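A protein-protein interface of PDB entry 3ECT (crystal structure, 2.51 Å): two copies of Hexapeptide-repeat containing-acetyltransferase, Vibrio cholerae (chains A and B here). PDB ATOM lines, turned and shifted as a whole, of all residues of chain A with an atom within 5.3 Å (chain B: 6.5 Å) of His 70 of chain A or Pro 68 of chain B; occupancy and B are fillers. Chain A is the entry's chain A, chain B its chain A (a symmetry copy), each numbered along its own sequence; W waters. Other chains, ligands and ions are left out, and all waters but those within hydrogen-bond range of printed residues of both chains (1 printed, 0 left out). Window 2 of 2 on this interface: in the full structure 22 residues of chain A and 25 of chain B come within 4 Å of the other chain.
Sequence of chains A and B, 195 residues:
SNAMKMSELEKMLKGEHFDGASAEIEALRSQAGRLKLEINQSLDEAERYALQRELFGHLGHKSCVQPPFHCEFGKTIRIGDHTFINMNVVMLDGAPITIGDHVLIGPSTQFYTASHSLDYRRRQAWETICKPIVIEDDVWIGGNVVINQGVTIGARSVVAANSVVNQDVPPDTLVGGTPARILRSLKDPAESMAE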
ATOM      1  N   LYS A  36       7.106  -9.153 -27.819  1.00  0.00           N
ATOM      2  CA  LYS A  36       7.026  -8.401 -26.575  1.00  0.00           C
ATOM      3  C   LYS A  36       6.571  -7.004 -26.912  1.00  0.00           C
ATOM      4  O   LYS A  36       5.558  -6.524 -26.427  1.00  0.00           O
ATOM      5  CB  LYS A  36       8.424  -8.329 -25.989  1.00  0.00           C
ATOM      6  CG  LYS A  36       8.562  -8.751 -24.573  1.00  0.00           C
ATOM      7  CD  LYS A  36       9.979  -9.174 -24.294  1.00  0.00           C
ATOM      8  CE  LYS A  36      10.993  -8.382 -25.113  1.00  0.00           C
ATOM      9  NZ  LYS A  36      12.350  -8.438 -24.541  1.00  0.00           N
ATOM     10  N   ASN A  40       3.192  -5.323 -25.679  1.00  0.00           N
ATOM     11  CA  ASN A  40       3.237  -4.145 -24.815  1.00  0.00           C
ATOM     12  C   ASN A  40       2.659  -2.926 -25.513  1.00  0.00           C
ATOM     13  O   ASN A  40       2.247  -1.988 -24.860  1.00  0.00           O
ATOM     14  CB  ASN A  40       4.667  -3.856 -24.317  1.00  0.00           C
ATOM     15  CG  ASN A  40       5.290  -5.039 -23.541  1.00  0.00           C
ATOM     16  OD1 ASN A  40       4.593  -5.902 -23.005  1.00  0.00           O
ATOM     17  ND2 ASN A  40       6.619  -5.062 -23.482  1.00  0.00           N
ATOM     18  N   PRO A  68       3.180  -3.527 -19.352  1.00  0.00           N
ATOM     19  CA  PRO A  68       4.270  -4.141 -20.133  1.00  0.00           C
ATOM     20  C   PRO A  68       4.764  -5.370 -19.425  1.00  0.00           C
ATOM     21  O   PRO A  68       4.827  -5.395 -18.192  1.00  0.00           O
ATOM     22  CB  PRO A  68       5.374  -3.071 -20.127  1.00  0.00           C
ATOM     23  CG  PRO A  68       5.103  -2.291 -18.921  1.00  0.00           C
ATOM     24  CD  PRO A  68       3.615  -2.259 -18.737  1.00  0.00           C
ATOM     25  N   PHE A  69       5.111  -6.392 -20.190  1.00  0.00           N
ATOM     26  CA  PHE A  69       5.696  -7.592 -19.622  1.00  0.00           C
ATOM     27  C   PHE A  69       7.043  -7.835 -20.320  1.00  0.00           C
ATOM     28  O   PHE A  69       7.154  -7.667 -21.531  1.00  0.00           O
ATOM     29  CB  PHE A  69       4.714  -8.746 -19.799  1.00  0.00           C
ATOM     30  CG  PHE A  69       5.308 -10.074 -19.563  1.00  0.00           C
ATOM     31  CD1 PHE A  69       5.955 -10.738 -20.594  1.00  0.00           C
ATOM     32  CD2 PHE A  69       5.224 -10.681 -18.297  1.00  0.00           C
ATOM     33  CE1 PHE A  69       6.509 -11.984 -20.374  1.00  0.00           C
ATOM     34  CE2 PHE A  69       5.784 -11.934 -18.053  1.00  0.00           C
ATOM     35  CZ  PHE A  69       6.426 -12.579 -19.094  1.00  0.00           C
ATOM     36  N   HIS A  70       8.061  -8.217 -19.543  1.00  0.00           N
ATOM     37  CA  HIS A  70       9.422  -8.440 -20.072  1.00  0.00           C
ATOM     38  C   HIS A  70      10.018  -9.822 -19.841  1.00  0.00           C
ATOM     39  O   HIS A  70      10.013 -10.362 -18.715  1.00  0.00           O
ATOM     40  CB  HIS A  70      10.366  -7.389 -19.542  1.00  0.00           C
ATOM     41  CG  HIS A  70       9.894  -6.003 -19.819  1.00  0.00           C
ATOM     42  ND1 HIS A  70       9.898  -5.456 -21.091  1.00  0.00           N
ATOM     43  CD2 HIS A  70       9.341  -5.075 -19.003  1.00  0.00           C
ATOM     44  CE1 HIS A  70       9.396  -4.233 -21.035  1.00  0.00           C
ATOM     45  NE2 HIS A  70       9.058  -3.977 -19.780  1.00  0.00           N
ATOM     46  N   CYS A  71      10.532 -10.396 -20.914  1.00  0.00           N
ATOM     47  CA  CYS A  71      11.302 -11.618 -20.815  1.00  0.00           C
ATOM     48  C   CYS A  71      12.250 -11.696 -21.976  1.00  0.00           C
ATOM     49  O   CYS A  71      12.236 -10.835 -22.870  1.00  0.00           O
ATOM     50  CB  CYS A  71      10.389 -12.826 -20.832  1.00  0.00           C
ATOM     51  SG  CYS A  71       9.386 -12.930 -22.361  1.00  0.00           S
ATOM     52  N   GLU A  72      13.077 -12.735 -21.957  1.00  0.00           N
ATOM     53  CA  GLU A  72      14.079 -12.882 -22.978  1.00  0.00           C
ATOM     54  C   GLU A  72      13.622 -13.850 -24.052  1.00  0.00           C
ATOM     55  O   GLU A  72      13.664 -13.502 -25.231  1.00  0.00           O
ATOM     56  CB  GLU A  72      15.439 -13.279 -22.387  1.00  0.00           C
ATOM     57  CG  GLU A  72      16.607 -12.879 -23.331  1.00  0.00           C
ATOM     58  CD  GLU A  72      18.013 -13.342 -22.870  1.00  0.00           C
ATOM     59  OE1 GLU A  72      18.922 -13.513 -23.761  1.00  0.00           O
ATOM     60  OE2 GLU A  72      18.197 -13.507 -21.622  1.00  0.00           O
ATOM     61  N   ASN A  88       4.299  -4.971 -15.596  1.00  0.00           N
ATOM     62  CA  ASN A  88       5.714  -4.671 -15.335  1.00  0.00           C
ATOM     63  C   ASN A  88       6.536  -5.832 -14.720  1.00  0.00           C
ATOM     64  O   ASN A  88       7.549  -5.632 -14.051  1.00  0.00           O
ATOM     65  CB  ASN A  88       5.826  -3.363 -14.542  1.00  0.00           C
ATOM     66  CG  ASN A  88       7.154  -2.669 -14.756  1.00  0.00           C
ATOM     67  OD1 ASN A  88       7.788  -2.820 -15.812  1.00  0.00           O
ATOM     68  ND2 ASN A  88       7.608  -1.933 -13.747  1.00  0.00           N
ATOM     69  N   VAL A  89       6.091  -7.060 -14.977  1.00  0.00           N
ATOM     70  CA  VAL A  89       6.840  -8.225 -14.561  1.00  0.00           C
ATOM     71  C   VAL A  89       8.018  -8.550 -15.518  1.00  0.00           C
ATOM     72  O   VAL A  89       7.909  -8.457 -16.770  1.00  0.00           O
ATOM     73  CB  VAL A  89       5.892  -9.437 -14.302  1.00  0.00           C
ATOM     74  CG1 VAL A  89       6.660 -10.758 -14.234  1.00  0.00           C
ATOM     75  CG2 VAL A  89       5.046  -9.165 -13.017  1.00  0.00           C
ATOM     76  N   VAL A  90       9.144  -8.902 -14.901  1.00  0.00           N
ATOM     77  CA  VAL A  90      10.353  -9.268 -15.615  1.00  0.00           C
ATOM     78  C   VAL A  90      10.663 -10.748 -15.378  1.00  0.00           C
ATOM     79  O   VAL A  90      10.693 -11.185 -14.232  1.00  0.00           O
ATOM     80  CB  VAL A  90      11.571  -8.375 -15.211  1.00  0.00           C
ATOM     81  CG1 VAL A  90      12.893  -8.978 -15.721  1.00  0.00           C
ATOM     82  CG2 VAL A  90      11.385  -6.929 -15.733  1.00  0.00           C
ATOM     83  N   MET A  91      10.884 -11.506 -16.461  1.00  0.00           N
ATOM     84  CA  MET A  91      11.280 -12.918 -16.334  1.00  0.00           C
ATOM     85  C   MET A  91      12.540 -13.269 -17.131  1.00  0.00           C
ATOM     86  O   MET A  91      12.514 -13.309 -18.368  1.00  0.00           O
ATOM     87  CB  MET A  91      10.135 -13.867 -16.719  1.00  0.00           C
ATOM     88  CG  MET A  91       8.831 -13.629 -15.996  1.00  0.00           C
ATOM     89  SD  MET A  91       7.566 -15.152 -16.033  1.00  0.00           S
ATOM     90  CE  MET A  91       7.095 -15.211 -17.895  1.00  0.00           C
ATOM     91  N   ASN B  40      14.427   1.826 -27.079  1.00  0.00           N
ATOM     92  CA  ASN B  40      13.489   0.881 -26.476  1.00  0.00           C
ATOM     93  C   ASN B  40      12.496   0.359 -27.499  1.00  0.00           C
ATOM     94  O   ASN B  40      11.920  -0.693 -27.307  1.00  0.00           O
ATOM     95  CB  ASN B  40      12.751   1.498 -25.270  1.00  0.00           C
ATOM     96  CG  ASN B  40      13.707   1.993 -24.162  1.00  0.00           C
ATOM     97  OD1 ASN B  40      14.852   1.550 -24.046  1.00  0.00           O
ATOM     98  ND2 ASN B  40      13.217   2.916 -23.339  1.00  0.00           N
ATOM     99  N   GLN B  66      20.406  -3.976 -22.768  1.00  0.00           N
ATOM    100  CA  GLN B  66      19.101  -4.528 -23.168  1.00  0.00           C
ATOM    101  C   GLN B  66      17.916  -3.602 -22.931  1.00  0.00           C
ATOM    102  O   GLN B  66      17.743  -3.063 -21.845  1.00  0.00           O
ATOM    103  CB  GLN B  66      18.814  -5.794 -22.382  1.00  0.00           C
ATOM    104  CG  GLN B  66      19.784  -6.904 -22.597  1.00  0.00           C
ATOM    105  CD  GLN B  66      19.758  -7.404 -24.026  1.00  0.00           C
ATOM    106  OE1 GLN B  66      19.009  -6.914 -24.863  1.00  0.00           O
ATOM    107  NE2 GLN B  66      20.586  -8.377 -24.316  1.00  0.00           N
ATOM    108  N   PRO B  67      17.049  -3.439 -23.923  1.00  0.00           N
ATOM    109  CA  PRO B  67      15.895  -2.584 -23.648  1.00  0.00           C
ATOM    110  C   PRO B  67      14.789  -3.283 -22.810  1.00  0.00           C
ATOM    111  O   PRO B  67      14.766  -4.513 -22.755  1.00  0.00           O
ATOM    112  CB  PRO B  67      15.402  -2.248 -25.049  1.00  0.00           C
ATOM    113  CG  PRO B  67      15.753  -3.479 -25.829  1.00  0.00           C
ATOM    114  CD  PRO B  67      17.064  -3.930 -25.311  1.00  0.00           C
ATOM    115  N   PRO B  68      13.875  -2.508 -22.163  1.00  0.00           N
ATOM    116  CA  PRO B  68      13.871  -1.035 -22.096  1.00  0.00           C
ATOM    117  C   PRO B  68      14.909  -0.574 -21.113  1.00  0.00           C
ATOM    118  O   PRO B  68      15.114  -1.217 -20.078  1.00  0.00           O
ATOM    119  CB  PRO B  68      12.471  -0.695 -21.558  1.00  0.00           C
ATOM    120  CG  PRO B  68      12.075  -1.895 -20.822  1.00  0.00           C
ATOM    121  CD  PRO B  68      12.662  -3.072 -21.542  1.00  0.00           C
ATOM    122  N   PHE B  69      15.567   0.530 -21.424  1.00  0.00           N
ATOM    123  CA  PHE B  69      16.518   1.123 -20.503  1.00  0.00           C
ATOM    124  C   PHE B  69      16.091   2.579 -20.257  1.00  0.00           C
ATOM    125  O   PHE B  69      15.692   3.272 -21.188  1.00  0.00           O
ATOM    126  CB  PHE B  69      17.917   1.003 -21.100  1.00  0.00           C
ATOM    127  CG  PHE B  69      18.925   1.842 -20.429  1.00  0.00           C
ATOM    128  CD1 PHE B  69      19.097   3.161 -20.816  1.00  0.00           C
ATOM    129  CD2 PHE B  69      19.720   1.317 -19.394  1.00  0.00           C
ATOM    130  CE1 PHE B  69      20.044   3.949 -20.189  1.00  0.00           C
ATOM    131  CE2 PHE B  69      20.675   2.098 -18.744  1.00  0.00           C
ATOM    132  CZ  PHE B  69      20.831   3.411 -19.145  1.00  0.00           C
ATOM    133  N   HIS B  70      16.169   3.022 -19.000  1.00  0.00           N
ATOM    134  CA  HIS B  70      15.747   4.384 -18.612  1.00  0.00           C
ATOM    135  C   HIS B  70      16.803   5.251 -17.938  1.00  0.00           C
ATOM    136  O   HIS B  70      17.483   4.833 -16.977  1.00  0.00           O
ATOM    137  CB  HIS B  70      14.516   4.320 -17.742  1.00  0.00           C
ATOM    138  CG  HIS B  70      13.401   3.566 -18.381  1.00  0.00           C
ATOM    139  ND1 HIS B  70      12.691   4.061 -19.461  1.00  0.00           N
ATOM    140  CD2 HIS B  70      12.917   2.324 -18.139  1.00  0.00           C
ATOM    141  CE1 HIS B  70      11.791   3.166 -19.832  1.00  0.00           C
ATOM    142  NE2 HIS B  70      11.904   2.108 -19.042  1.00  0.00           N
ATOM    143  N   ASN B  86      21.423  -5.811 -18.265  1.00  0.00           N
ATOM    144  CA  ASN B  86      20.148  -6.437 -18.557  1.00  0.00           C
ATOM    145  C   ASN B  86      18.979  -5.452 -18.606  1.00  0.00           C
ATOM    146  O   ASN B  86      19.159  -4.267 -18.369  1.00  0.00           O
ATOM    147  CB  ASN B  86      19.876  -7.520 -17.553  1.00  0.00           C
ATOM    148  CG  ASN B  86      19.296  -8.787 -18.192  1.00  0.00           C
ATOM    149  OD1 ASN B  86      19.589  -9.896 -17.726  1.00  0.00           O
ATOM    150  ND2 ASN B  86      18.460  -8.633 -19.232  1.00  0.00           N
ATOM    151  N   MET B  87      17.779  -5.938 -18.919  1.00  0.00           N
ATOM    152  CA  MET B  87      16.657  -5.044 -19.232  1.00  0.00           C
ATOM    153  C   MET B  87      16.101  -4.320 -18.037  1.00  0.00           C
ATOM    154  O   MET B  87      16.323  -4.711 -16.882  1.00  0.00           O
ATOM    155  CB  MET B  87      15.537  -5.777 -19.967  1.00  0.00           C
ATOM    156  CG  MET B  87      15.302  -7.173 -19.465  1.00  0.00           C
ATOM    157  SD  MET B  87      14.184  -8.289 -20.661  1.00  0.00           S
ATOM    158  CE  MET B  87      14.323  -9.926 -19.589  1.00  0.00           C
ATOM    159  N   ASN B  88      15.376  -3.239 -18.335  1.00  0.00           N
ATOM    160  CA  ASN B  88      14.593  -2.503 -17.331  1.00  0.00           C
ATOM    161  C   ASN B  88      15.424  -1.784 -16.238  1.00  0.00           C
ATOM    162  O   ASN B  88      14.959  -1.523 -15.130  1.00  0.00           O
ATOM    163  CB  ASN B  88      13.500  -3.414 -16.759  1.00  0.00           C
ATOM    164  CG  ASN B  88      12.316  -2.635 -16.230  1.00  0.00           C
ATOM    165  OD1 ASN B  88      12.026  -1.523 -16.698  1.00  0.00           O
ATOM    166  ND2 ASN B  88      11.643  -3.188 -15.226  1.00  0.00           N
ATOM    167  N   VAL B  89      16.666  -1.446 -16.579  1.00  0.00           N
ATOM    168  CA  VAL B  89      17.495  -0.665 -15.689  1.00  0.00           C
ATOM    169  C   VAL B  89      17.166   0.851 -15.743  1.00  0.00           C
ATOM    170  O   VAL B  89      16.914   1.444 -16.826  1.00  0.00           O
ATOM    171  CB  VAL B  89      19.007  -0.985 -15.909  1.00  0.00           C
ATOM    172  CG1 VAL B  89      19.912   0.072 -15.272  1.00  0.00           C
ATOM    173  CG2 VAL B  89      19.311  -2.427 -15.392  1.00  0.00           C
ATOM    174  N   VAL B  90      17.147   1.450 -14.555  1.00  0.00           N
ATOM    175  CA  VAL B  90      16.884   2.867 -14.389  1.00  0.00           C
ATOM    176  C   VAL B  90      18.140   3.567 -13.867  1.00  0.00           C
ATOM    177  O   VAL B  90      18.717   3.120 -12.880  1.00  0.00           O
ATOM    178  CB  VAL B  90      15.666   3.136 -13.446  1.00  0.00           C
ATOM    179  CG1 VAL B  90      15.606   4.617 -13.027  1.00  0.00           C
ATOM    180  CG2 VAL B  90      14.343   2.699 -14.122  1.00  0.00           C
HETATM  181  O   HOH W   1      11.977  -5.807 -23.240  1.00  0.00           O
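The side-chain amino group (NZ) of Lys 36 of chain A lies within hydrogen-bond range of the backbone carbonyl oxygen (O) of Cys 71 of chain A.
The backbone carbonyl oxygen (O) of Pro 68 of chain A lies within hydrogen-bond range of the backbone NH (N) of Asn 88 of chain A (2.7 Å).
The backbone NH (N) of His 70 of chain A sits at hydrogen-bond distance from the backbone carbonyl oxygen (O) of Val 89 of chain A.
The backbone carbonyl oxygen (O) of His 70 of chain A sits at hydrogen-bond distance from the backbone NH (N) of Met 91 of chain A, 2.7 Å away.
O of Pro 68 of chain B is in hydrogen-bond range of N of Asn 88 of chain B (2.7 Å).
Water W1 lies within hydrogen-bond range of the side-chain amino group (NZ) of Lys 36 of chain A (3.0 Å), a ring nitrogen (ND1) of His 70 of chain A (3.0 Å) and the backbone carbonyl oxygen (O) of Pro 67 of chain B (3.1 Å).
Phe 69 of chain A touches none of the printed residues of chain B.
Of the printed residues of chain B, Glu 72 of chain A touches Met 87.
Val 89 of chain A touches none of the printed residues of chain B.
Printed residues of chain B within 4 Å of Val 90 of chain A: Asn 88 (3.8 Å).
Of chain A, only His 70 (3.5 Å) comes within 4 Å of Pro 68 of chain B.
Of the printed residues of chain A, Met 87 of chain B touches Cys 71 and Glu 72.
Of the printed residues of chain A, Asn 88 of chain B touches Asn 88 and Val 90.
The nearest printed residue of chain A that does not touch Pro 68 of chain B is Lys 36 of chain A (6.2 Å).
Hydrophobic or aromatic side chains of chain B that line the printed part of chain A: Pro 68 and Met 87.
Hydrophobic or aromatic side chains of chain A that line the printed part of chain B: His 70 and Val 90.
Among the printed residues, 5 pairs touch across the chains.
Among the printed residues, no Asp or Glu carboxylate lies within 4 Å of a Lys or Arg side-chain nitrogen of the other chain.
His 70 of chain A touches Pro 68 of chain B, but with the chains exchanged Pro 68 of chain A does not touch His 70 of chain B (8.1 Å).
Asn 88 of chain B touches its own counterpart, Asn 88 of chain A.
Val 90 of chain A touches Asn 88 of chain B, but with the chains exchanged Asn 88 of chain A does not touch Val 90 of chain B (8.2 Å).
Positions printed for both chains: 40, 68, 69, 70, 88, 89 and 90.
Of the 5 pairs that touch across the chains among the printed residues, 1 has its exchanged pair printed and touching as well.
Among the printed residues, pairs that only touch across the chains: His 70 of chain A with Pro 68 of chain B (3.5 Å), Cys 71 of chain A with Met 87 of chain B (3.6 Å), Glu 72 of chain A with Met 87 of chain B (3.9 Å), Asn 88 of chain A with Asn 88 of chain B (3.9 Å) and Val 90 of chain A with Asn 88 of chain B (3.8 Å).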
